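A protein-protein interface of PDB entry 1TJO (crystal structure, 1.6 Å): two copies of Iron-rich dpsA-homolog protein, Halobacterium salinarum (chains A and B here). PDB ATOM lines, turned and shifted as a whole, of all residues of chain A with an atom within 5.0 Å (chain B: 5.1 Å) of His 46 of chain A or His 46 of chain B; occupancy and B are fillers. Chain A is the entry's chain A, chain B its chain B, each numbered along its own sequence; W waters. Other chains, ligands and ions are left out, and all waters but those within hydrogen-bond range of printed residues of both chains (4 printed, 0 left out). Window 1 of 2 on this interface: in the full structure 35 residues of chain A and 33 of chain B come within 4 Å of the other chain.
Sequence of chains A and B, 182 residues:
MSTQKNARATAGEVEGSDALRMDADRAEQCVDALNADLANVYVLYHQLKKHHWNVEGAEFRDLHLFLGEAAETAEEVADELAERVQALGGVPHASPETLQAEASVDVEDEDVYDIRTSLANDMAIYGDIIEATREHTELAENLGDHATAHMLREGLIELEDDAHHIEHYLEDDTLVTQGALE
The side-chain hydroxyl (OH) of Tyr 45 of chain B lies within hydrogen-bond range of the side-chain hydroxyl (OH) of Tyr 42 of chain A, 2.8 Å away. NE2 of His 46 of chain A is in hydrogen-bond range of NE2 of His 46 of chain B (2.8 Å). OH of Tyr 42 of chain B is in hydrogen-bond range of OH of Tyr 45 of chain A (2.7 Å).
Tyr 42 of chain A touches His 46 of chain B, and with the chains exchanged His 46 of chain A touches Tyr 42 of chain B. Tyr 42 of chain A touches Lys 49 of chain B, and with the chains exchanged Lys 49 of chain A touches Tyr 42 of chain B. Lys 50 of chain A touches Ala 94 of chain B, and with the chains exchanged Ala 94 of chain A touches Lys 50 of chain B. Pro 96 of chain B touches its own counterpart, Pro 96 of chain A. 13 positions are printed for both chains. Of the 16 pairs that touch across the chains among the printed residues, 16 have their exchanged pair printed and touching as well.
CE2 of Tyr 42 of chain A touches CE1 of His 46 of chain B, at 3.5 Å. Tyr 42 of chain A touches Lys 49 of chain B (OH to CE, 3.9 Å). Tyr 42 of chain B touches His 46 of chain A. CB of His 46 of chain A touches O of Ala 94 of chain B, 3.6 Å away. His 46 of chain A touches Pro 96 of chain B (CD2 to CG, 3.7 Å). CE1 of His 46 of chain A touches CD1 of Leu 99 of chain B, at 3.6 Å. Lys 50 of chain A touches Ala 94 of chain B. Ala 94 of chain A touches His 46 of chain B (O to CB, 3.7 Å). Ala 94 of chain A touches Lys 50 of chain B. Leu 99 of chain A touches His 46 of chain B.
Water W4 lies within hydrogen-bond range of the backbone carbonyl oxygen of Ala 94 of chain A (2.6 Å) and a ring nitrogen (ND1) of His 46 of chain B (2.7 Å). Water W2 lies within hydrogen-bond range of the side-chain hydroxyl (OH) of Tyr 42 of chain A and the side-chain amino group (NZ) of Lys 49 of chain B. Water W3 lies within hydrogen-bond range of O of Ala 94 of chain B and ND1 of His 46 of chain A. Water W1 lies within hydrogen-bond range of the side-chain hydroxyl (OH) of Tyr 42 of chain B (2.7 Å) and the side-chain amino group (NZ) of Lys 49 of chain A (3.0 Å).
Of the printed residues of chain B, His 46 of chain A touches Tyr 42, His 46, Ala 94, Pro 96 and Leu 99. Of chain A, only Tyr 42, His 46, Ala 94, Pro 96 and Leu 99 come within 4 Å of His 46 of chain B. Printed residues of chain B within 4 Å of Tyr 42 of chain A: Tyr 45, His 46 and Lys 49. Printed residues of chain A within 4 Å of Tyr 42 of chain B: Tyr 45 (2.7 Å), His 46 (3.6 Å) and Lys 49 (3.8 Å). Printed residues of chain A within 4 Å of Tyr 45 of chain B: Tyr 42 (2.8 Å).
Printed residues of chain A that touch a printed residue of chain B: Tyr 42, Tyr 45, His 46, Lys 49, Lys 50, Ala 94, Pro 96 and Leu 99. Hydrophobic or aromatic side chains of chain A that line the printed part of chain B: Tyr 42, Tyr 45, His 46, Ala 94, Pro 96 and Leu 99. Of the 13 printed residues of chain B, 8 touch a printed residue of chain A. Among the printed residues, 16 pairs touch across the chains. Among the printed residues, no Asp or Glu carboxylate lies within 4 Å of a Lys or Arg side-chain nitrogen of the other chain.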
ATOM      1  N   TYR A  42     -18.857  36.057  22.421  1.00  0.00           N
ATOM      2  CA  TYR A  42     -19.042  34.670  22.020  1.00  0.00           C
ATOM      3  C   TYR A  42     -17.823  34.056  21.295  1.00  0.00           C
ATOM      4  O   TYR A  42     -17.537  32.887  21.461  1.00  0.00           O
ATOM      5  CB  TYR A  42     -20.348  34.427  21.248  1.00  0.00           C
ATOM      6  CG  TYR A  42     -21.385  33.689  22.120  1.00  0.00           C
ATOM      7  CD1 TYR A  42     -22.678  34.140  22.190  1.00  0.00           C
ATOM      8  CD2 TYR A  42     -21.059  32.519  22.787  1.00  0.00           C
ATOM      9  CE1 TYR A  42     -23.619  33.501  22.934  1.00  0.00           C
ATOM     10  CE2 TYR A  42     -22.006  31.867  23.549  1.00  0.00           C
ATOM     11  CZ  TYR A  42     -23.283  32.363  23.614  1.00  0.00           C
ATOM     12  OH  TYR A  42     -24.251  31.727  24.395  1.00  0.00           O
ATOM     13  N   VAL A  43     -17.096  34.873  20.532  1.00  0.00           N
ATOM     14  CA  VAL A  43     -15.825  34.441  19.972  1.00  0.00           C
ATOM     15  C   VAL A  43     -14.822  34.152  21.102  1.00  0.00           C
ATOM     16  O   VAL A  43     -14.146  33.144  21.073  1.00  0.00           O
ATOM     17  CB  VAL A  43     -15.234  35.401  18.898  1.00  0.00           C
ATOM     18  CG1 VAL A  43     -16.121  35.395  17.649  1.00  0.00           C
ATOM     19  CG2 VAL A  43     -15.112  36.739  19.394  1.00  0.00           C
ATOM     20  N   LEU A  44     -14.791  35.010  22.124  1.00  0.00           N
ATOM     21  CA  LEU A  44     -13.951  34.816  23.293  1.00  0.00           C
ATOM     22  C   LEU A  44     -14.315  33.503  23.973  1.00  0.00           C
ATOM     23  O   LEU A  44     -13.457  32.684  24.266  1.00  0.00           O
ATOM     24  CB  LEU A  44     -14.093  35.993  24.270  1.00  0.00           C
ATOM     25  CG  LEU A  44     -13.371  35.777  25.606  1.00  0.00           C
ATOM     26  CD1 LEU A  44     -11.867  35.674  25.384  1.00  0.00           C
ATOM     27  CD2 LEU A  44     -13.796  36.863  26.595  1.00  0.00           C
ATOM     28  N   TYR A  45     -15.603  33.329  24.215  1.00  0.00           N
ATOM     29  CA  TYR A  45     -16.097  32.102  24.846  1.00  0.00           C
ATOM     30  C   TYR A  45     -15.570  30.872  24.091  1.00  0.00           C
ATOM     31  O   TYR A  45     -15.040  29.889  24.701  1.00  0.00           O
ATOM     32  CB  TYR A  45     -17.629  32.076  24.812  1.00  0.00           C
ATOM     33  CG  TYR A  45     -18.257  30.707  25.078  1.00  0.00           C
ATOM     34  CD1 TYR A  45     -18.380  30.223  26.349  1.00  0.00           C
ATOM     35  CD2 TYR A  45     -18.731  29.955  24.029  1.00  0.00           C
ATOM     36  CE1 TYR A  45     -18.958  28.986  26.576  1.00  0.00           C
ATOM     37  CE2 TYR A  45     -19.264  28.718  24.208  1.00  0.00           C
ATOM     38  CZ  TYR A  45     -19.421  28.246  25.488  1.00  0.00           C
ATOM     39  OH  TYR A  45     -19.991  27.000  25.671  1.00  0.00           O
ATOM     40  N   HIS A  46     -15.733  30.879  22.765  1.00  0.00           N
ATOM     41  CA  HIS A  46     -15.342  29.698  21.992  1.00  0.00           C
ATOM     42  C   HIS A  46     -13.834  29.452  21.990  1.00  0.00           C
ATOM     43  O   HIS A  46     -13.379  28.305  21.998  1.00  0.00           O
ATOM     44  CB  HIS A  46     -15.889  29.773  20.570  1.00  0.00           C
ATOM     45  CG  HIS A  46     -17.283  29.267  20.482  1.00  0.00           C
ATOM     46  ND1 HIS A  46     -17.576  27.933  20.639  1.00  0.00           N
ATOM     47  CD2 HIS A  46     -18.475  29.903  20.311  1.00  0.00           C
ATOM     48  CE1 HIS A  46     -18.892  27.769  20.541  1.00  0.00           C
ATOM     49  NE2 HIS A  46     -19.453  28.943  20.354  1.00  0.00           N
ATOM     50  N   GLN A  47     -13.050  30.522  22.063  1.00  0.00           N
ATOM     51  CA  GLN A  47     -11.594  30.381  22.093  1.00  0.00           C
ATOM     52  C   GLN A  47     -11.082  29.969  23.478  1.00  0.00           C
ATOM     53  O   GLN A  47     -10.143  29.187  23.588  1.00  0.00           O
ATOM     54  CB  GLN A  47     -10.929  31.662  21.684  1.00  0.00           C
ATOM     55  CG  GLN A  47      -9.443  31.465  21.430  1.00  0.00           C
ATOM     56  CD  GLN A  47      -8.859  32.458  20.429  1.00  0.00           C
ATOM     57  OE1 GLN A  47      -9.135  32.367  19.232  1.00  0.00           O
ATOM     58  NE2 GLN A  47      -8.062  33.409  20.920  1.00  0.00           N
ATOM     59  N   LEU A  48     -11.776  30.421  24.517  1.00  0.00           N
ATOM     60  CA  LEU A  48     -11.472  29.980  25.880  1.00  0.00           C
ATOM     61  C   LEU A  48     -11.769  28.489  25.989  1.00  0.00           C
ATOM     62  O   LEU A  48     -10.999  27.733  26.586  1.00  0.00           O
ATOM     63  CB  LEU A  48     -12.285  30.768  26.904  1.00  0.00           C
ATOM     64  CG  LEU A  48     -11.893  32.218  27.085  1.00  0.00           C
ATOM     65  CD1 LEU A  48     -12.856  32.943  27.963  1.00  0.00           C
ATOM     66  CD2 LEU A  48     -10.495  32.399  27.658  1.00  0.00           C
ATOM     67  N   LYS A  49     -12.900  28.078  25.424  1.00  0.00           N
ATOM     68  CA  LYS A  49     -13.230  26.646  25.380  1.00  0.00           C
ATOM     69  C   LYS A  49     -12.160  25.858  24.677  1.00  0.00           C
ATOM     70  O   LYS A  49     -11.700  24.883  25.196  1.00  0.00           O
ATOM     71  CB  LYS A  49     -14.584  26.393  24.712  1.00  0.00           C
ATOM     72  CG  LYS A  49     -15.820  26.773  25.544  1.00  0.00           C
ATOM     73  CD  LYS A  49     -15.832  26.112  26.864  1.00  0.00           C
ATOM     74  CE  LYS A  49     -16.235  24.717  26.832  1.00  0.00           C
ATOM     75  NZ  LYS A  49     -17.200  24.412  28.021  1.00  0.00           N
ATOM     76  N   LYS A  50     -11.711  26.317  23.507  1.00  0.00           N
ATOM     77  CA  LYS A  50     -10.630  25.660  22.797  1.00  0.00           C
ATOM     78  C   LYS A  50      -9.407  25.481  23.685  1.00  0.00           C
ATOM     79  O   LYS A  50      -8.815  24.418  23.751  1.00  0.00           O
ATOM     80  CB  LYS A  50     -10.213  26.516  21.616  1.00  0.00           C
ATOM     81  CG  LYS A  50      -9.062  25.941  20.859  1.00  0.00           C
ATOM     82  CD  LYS A  50      -8.752  26.837  19.675  1.00  0.00           C
ATOM     83  CE  LYS A  50      -7.617  26.261  18.881  1.00  0.00           C
ATOM     84  NZ  LYS A  50      -7.131  27.132  17.752  1.00  0.00           N
ATOM     85  N   ALA A  94     -27.074  35.487  16.573  1.00  0.00           N
ATOM     86  CA  ALA A  94     -27.342  34.168  17.094  1.00  0.00           C
ATOM     87  C   ALA A  94     -26.494  33.050  16.532  1.00  0.00           C
ATOM     88  O   ALA A  94     -25.906  32.274  17.303  1.00  0.00           O
ATOM     89  CB  ALA A  94     -28.817  33.861  16.932  1.00  0.00           C
ATOM     90  N   SER A  95     -26.461  32.899  15.211  1.00  0.00           N
ATOM     91  CA  SER A  95     -25.747  31.752  14.652  1.00  0.00           C
ATOM     92  C   SER A  95     -24.266  31.923  14.833  1.00  0.00           C
ATOM     93  O   SER A  95     -23.782  33.035  14.874  1.00  0.00           O
ATOM     94  CB  SER A  95     -26.060  31.568  13.146  1.00  0.00           C
ATOM     95  OG  SER A  95     -25.469  32.550  12.305  1.00  0.00           O
ATOM     96  N   PRO A  96     -23.543  30.825  14.918  1.00  0.00           N
ATOM     97  CA  PRO A  96     -22.096  30.892  15.101  1.00  0.00           C
ATOM     98  C   PRO A  96     -21.432  31.681  13.967  1.00  0.00           C
ATOM     99  O   PRO A  96     -20.567  32.517  14.236  1.00  0.00           O
ATOM    100  CB  PRO A  96     -21.683  29.431  15.062  1.00  0.00           C
ATOM    101  CG  PRO A  96     -22.850  28.713  15.575  1.00  0.00           C
ATOM    102  CD  PRO A  96     -24.034  29.427  15.001  1.00  0.00           C
ATOM    103  N   LEU A  99     -22.132  35.413  14.624  1.00  0.00           N
ATOM    104  CA  LEU A  99     -21.329  35.915  15.735  1.00  0.00           C
ATOM    105  C   LEU A  99     -19.865  36.184  15.335  1.00  0.00           C
ATOM    106  O   LEU A  99     -19.325  37.246  15.633  1.00  0.00           O
ATOM    107  CB  LEU A  99     -21.397  34.907  16.894  1.00  0.00           C
ATOM    108  CG  LEU A  99     -22.738  34.814  17.610  1.00  0.00           C
ATOM    109  CD1 LEU A  99     -22.817  33.597  18.467  1.00  0.00           C
ATOM    110  CD2 LEU A  99     -22.995  36.104  18.423  1.00  0.00           C
ATOM    111  N   TYR B  42     -22.991  22.074  18.922  1.00  0.00           N
ATOM    112  CA  TYR B  42     -22.773  23.464  19.197  1.00  0.00           C
ATOM    113  C   TYR B  42     -23.702  24.357  18.378  1.00  0.00           C
ATOM    114  O   TYR B  42     -24.083  25.429  18.873  1.00  0.00           O
ATOM    115  CB  TYR B  42     -21.292  23.888  19.058  1.00  0.00           C
ATOM    116  CG  TYR B  42     -20.659  24.211  20.386  1.00  0.00           C
ATOM    117  CD1 TYR B  42     -19.438  23.724  20.740  1.00  0.00           C
ATOM    118  CD2 TYR B  42     -21.286  25.097  21.283  1.00  0.00           C
ATOM    119  CE1 TYR B  42     -18.855  24.058  21.961  1.00  0.00           C
ATOM    120  CE2 TYR B  42     -20.722  25.387  22.515  1.00  0.00           C
ATOM    121  CZ  TYR B  42     -19.506  24.866  22.829  1.00  0.00           C
ATOM    122  OH  TYR B  42     -18.875  25.158  24.039  1.00  0.00           O
ATOM    123  N   VAL B  43     -24.024  23.984  17.126  1.00  0.00           N
ATOM    124  CA  VAL B  43     -25.067  24.699  16.386  1.00  0.00           C
ATOM    125  C   VAL B  43     -26.396  24.619  17.091  1.00  0.00           C
ATOM    126  O   VAL B  43     -27.074  25.621  17.216  1.00  0.00           O
ATOM    127  CB  VAL B  43     -25.157  24.336  14.863  1.00  0.00           C
ATOM    128  CG1 VAL B  43     -23.900  24.805  14.164  1.00  0.00           C
ATOM    129  CG2 VAL B  43     -25.349  22.937  14.611  1.00  0.00           C
ATOM    130  N   LEU B  44     -26.745  23.448  17.611  1.00  0.00           N
ATOM    131  CA  LEU B  44     -27.920  23.238  18.415  1.00  0.00           C
ATOM    132  C   LEU B  44     -27.907  24.170  19.636  1.00  0.00           C
ATOM    133  O   LEU B  44     -28.890  24.903  19.872  1.00  0.00           O
ATOM    134  CB  LEU B  44     -28.032  21.788  18.884  1.00  0.00           C
ATOM    135  CG  LEU B  44     -29.194  21.501  19.826  1.00  0.00           C
ATOM    136  CD1 LEU B  44     -30.497  21.824  19.136  1.00  0.00           C
ATOM    137  CD2 LEU B  44     -29.109  20.079  20.300  1.00  0.00           C
ATOM    138  N   TYR B  45     -26.810  24.185  20.384  1.00  0.00           N
ATOM    139  CA  TYR B  45     -26.646  25.151  21.494  1.00  0.00           C
ATOM    140  C   TYR B  45     -26.942  26.584  21.147  1.00  0.00           C
ATOM    141  O   TYR B  45     -27.746  27.230  21.828  1.00  0.00           O
ATOM    142  CB  TYR B  45     -25.242  24.987  22.110  1.00  0.00           C
ATOM    143  CG  TYR B  45     -24.842  26.101  22.990  1.00  0.00           C
ATOM    144  CD1 TYR B  45     -25.195  26.132  24.337  1.00  0.00           C
ATOM    145  CD2 TYR B  45     -24.068  27.128  22.503  1.00  0.00           C
ATOM    146  CE1 TYR B  45     -24.754  27.154  25.139  1.00  0.00           C
ATOM    147  CE2 TYR B  45     -23.650  28.176  23.275  1.00  0.00           C
ATOM    148  CZ  TYR B  45     -23.988  28.200  24.611  1.00  0.00           C
ATOM    149  OH  TYR B  45     -23.557  29.225  25.406  1.00  0.00           O
ATOM    150  N   HIS B  46     -26.388  27.072  20.030  1.00  0.00           N
ATOM    151  CA  HIS B  46     -26.540  28.445  19.649  1.00  0.00           C
ATOM    152  C   HIS B  46     -27.963  28.763  19.256  1.00  0.00           C
ATOM    153  O   HIS B  46     -28.460  29.827  19.575  1.00  0.00           O
ATOM    154  CB  HIS B  46     -25.486  28.863  18.622  1.00  0.00           C
ATOM    155  CG  HIS B  46     -24.197  29.272  19.263  1.00  0.00           C
ATOM    156  ND1 HIS B  46     -24.061  30.457  19.958  1.00  0.00           N
ATOM    157  CD2 HIS B  46     -22.991  28.657  19.339  1.00  0.00           C
ATOM    158  CE1 HIS B  46     -22.827  30.555  20.430  1.00  0.00           C
ATOM    159  NE2 HIS B  46     -22.162  29.472  20.067  1.00  0.00           N
ATOM    160  N   GLN B  47     -28.623  27.830  18.615  1.00  0.00           N
ATOM    161  CA  GLN B  47     -30.023  28.023  18.181  1.00  0.00           C
ATOM    162  C   GLN B  47     -30.997  27.900  19.381  1.00  0.00           C
ATOM    163  O   GLN B  47     -31.960  28.647  19.479  1.00  0.00           O
ATOM    164  CB  GLN B  47     -30.402  27.068  17.071  1.00  0.00           C
ATOM    165  CG  GLN B  47     -31.755  27.363  16.492  1.00  0.00           C
ATOM    166  CD  GLN B  47     -31.905  26.963  15.045  1.00  0.00           C
ATOM    167  OE1 GLN B  47     -31.191  27.479  14.158  1.00  0.00           O
ATOM    168  NE2 GLN B  47     -32.754  25.974  14.807  1.00  0.00           N
ATOM    169  N   LEU B  48     -30.714  26.994  20.313  1.00  0.00           N
ATOM    170  CA  LEU B  48     -31.484  26.941  21.561  1.00  0.00           C
ATOM    171  C   LEU B  48     -31.348  28.258  22.338  1.00  0.00           C
ATOM    172  O   LEU B  48     -32.313  28.774  22.885  1.00  0.00           O
ATOM    173  CB  LEU B  48     -31.035  25.786  22.418  1.00  0.00           C
ATOM    174  CG  LEU B  48     -31.336  24.414  21.830  1.00  0.00           C
ATOM    175  CD1 LEU B  48     -30.683  23.398  22.693  1.00  0.00           C
ATOM    176  CD2 LEU B  48     -32.830  24.194  21.800  1.00  0.00           C
ATOM    177  N   LYS B  49     -30.131  28.819  22.382  1.00  0.00           N
ATOM    178  CA  LYS B  49     -29.912  30.132  22.995  1.00  0.00           C
ATOM    179  C   LYS B  49     -30.766  31.164  22.329  1.00  0.00           C
ATOM    180  O   LYS B  49     -31.390  31.994  22.985  1.00  0.00           O
ATOM    181  CB  LYS B  49     -28.445  30.539  23.006  1.00  0.00           C
ATOM    182  CG  LYS B  49     -27.592  29.771  23.969  1.00  0.00           C
ATOM    183  CD  LYS B  49     -27.997  29.881  25.416  1.00  0.00           C
ATOM    184  CE  LYS B  49     -27.706  31.134  26.064  1.00  0.00           C
ATOM    185  NZ  LYS B  49     -27.344  30.902  27.577  1.00  0.00           N
ATOM    186  N   LYS B  50     -30.739  31.174  21.006  1.00  0.00           N
ATOM    187  CA  LYS B  50     -31.528  32.123  20.211  1.00  0.00           C
ATOM    188  C   LYS B  50     -32.959  32.053  20.583  1.00  0.00           C
ATOM    189  O   LYS B  50     -33.567  33.086  20.883  1.00  0.00           O
ATOM    190  CB  LYS B  50     -31.412  31.785  18.741  1.00  0.00           C
ATOM    191  CG  LYS B  50     -32.150  32.741  17.842  1.00  0.00           C
ATOM    192  CD  LYS B  50     -32.187  32.206  16.439  1.00  0.00           C
ATOM    193  CE  LYS B  50     -33.025  33.114  15.542  1.00  0.00           C
ATOM    194  NZ  LYS B  50     -32.853  32.819  14.059  1.00  0.00           N
ATOM    195  N   ALA B  94     -13.326  24.290  16.958  1.00  0.00           N
ATOM    196  CA  ALA B  94     -13.326  25.287  17.998  1.00  0.00           C
ATOM    197  C   ALA B  94     -14.011  26.622  17.594  1.00  0.00           C
ATOM    198  O   ALA B  94     -14.875  27.131  18.300  1.00  0.00           O
ATOM    199  CB  ALA B  94     -11.921  25.521  18.466  1.00  0.00           C
ATOM    200  N   SER B  95     -13.607  27.236  16.487  1.00  0.00           N
ATOM    201  CA  SER B  95     -14.118  28.579  16.229  1.00  0.00           C
ATOM    202  C   SER B  95     -15.607  28.473  15.777  1.00  0.00           C
ATOM    203  O   SER B  95     -16.063  27.440  15.321  1.00  0.00           O
ATOM    204  CB  SER B  95     -13.270  29.289  15.191  1.00  0.00           C
ATOM    205  OG  SER B  95     -13.563  28.838  13.888  1.00  0.00           O
ATOM    206  N   PRO B  96     -16.394  29.516  16.023  1.00  0.00           N
ATOM    207  CA  PRO B  96     -17.814  29.506  15.628  1.00  0.00           C
ATOM    208  C   PRO B  96     -18.003  29.213  14.142  1.00  0.00           C
ATOM    209  O   PRO B  96     -18.804  28.347  13.784  1.00  0.00           O
ATOM    210  CB  PRO B  96     -18.316  30.917  16.029  1.00  0.00           C
ATOM    211  CG  PRO B  96     -17.413  31.333  17.093  1.00  0.00           C
ATOM    212  CD  PRO B  96     -16.041  30.709  16.798  1.00  0.00           C
ATOM    213  N   LEU B  99     -17.352  25.429  13.501  1.00  0.00           N
ATOM    214  CA  LEU B  99     -18.420  24.612  14.013  1.00  0.00           C
ATOM    215  C   LEU B  99     -19.609  24.674  13.068  1.00  0.00           C
ATOM    216  O   LEU B  99     -20.138  23.632  12.745  1.00  0.00           O
ATOM    217  CB  LEU B  99     -18.819  25.057  15.447  1.00  0.00           C
ATOM    218  CG  LEU B  99     -17.771  24.753  16.563  1.00  0.00           C
ATOM    219  CD1 LEU B  99     -17.938  25.609  17.772  1.00  0.00           C
ATOM    220  CD2 LEU B  99     -17.859  23.324  16.928  1.00  0.00           C
HETATM  221  O   HOH W   1     -18.805  23.131  25.772  1.00  0.00           O
HETATM  222  O   HOH W   2     -25.015  32.806  26.638  1.00  0.00           O
HETATM  223  O   HOH W   3     -15.221  26.397  20.777  1.00  0.00           O
HETATM  224  O   HOH W   4     -26.355  31.855  19.832  1.00  0.00           O
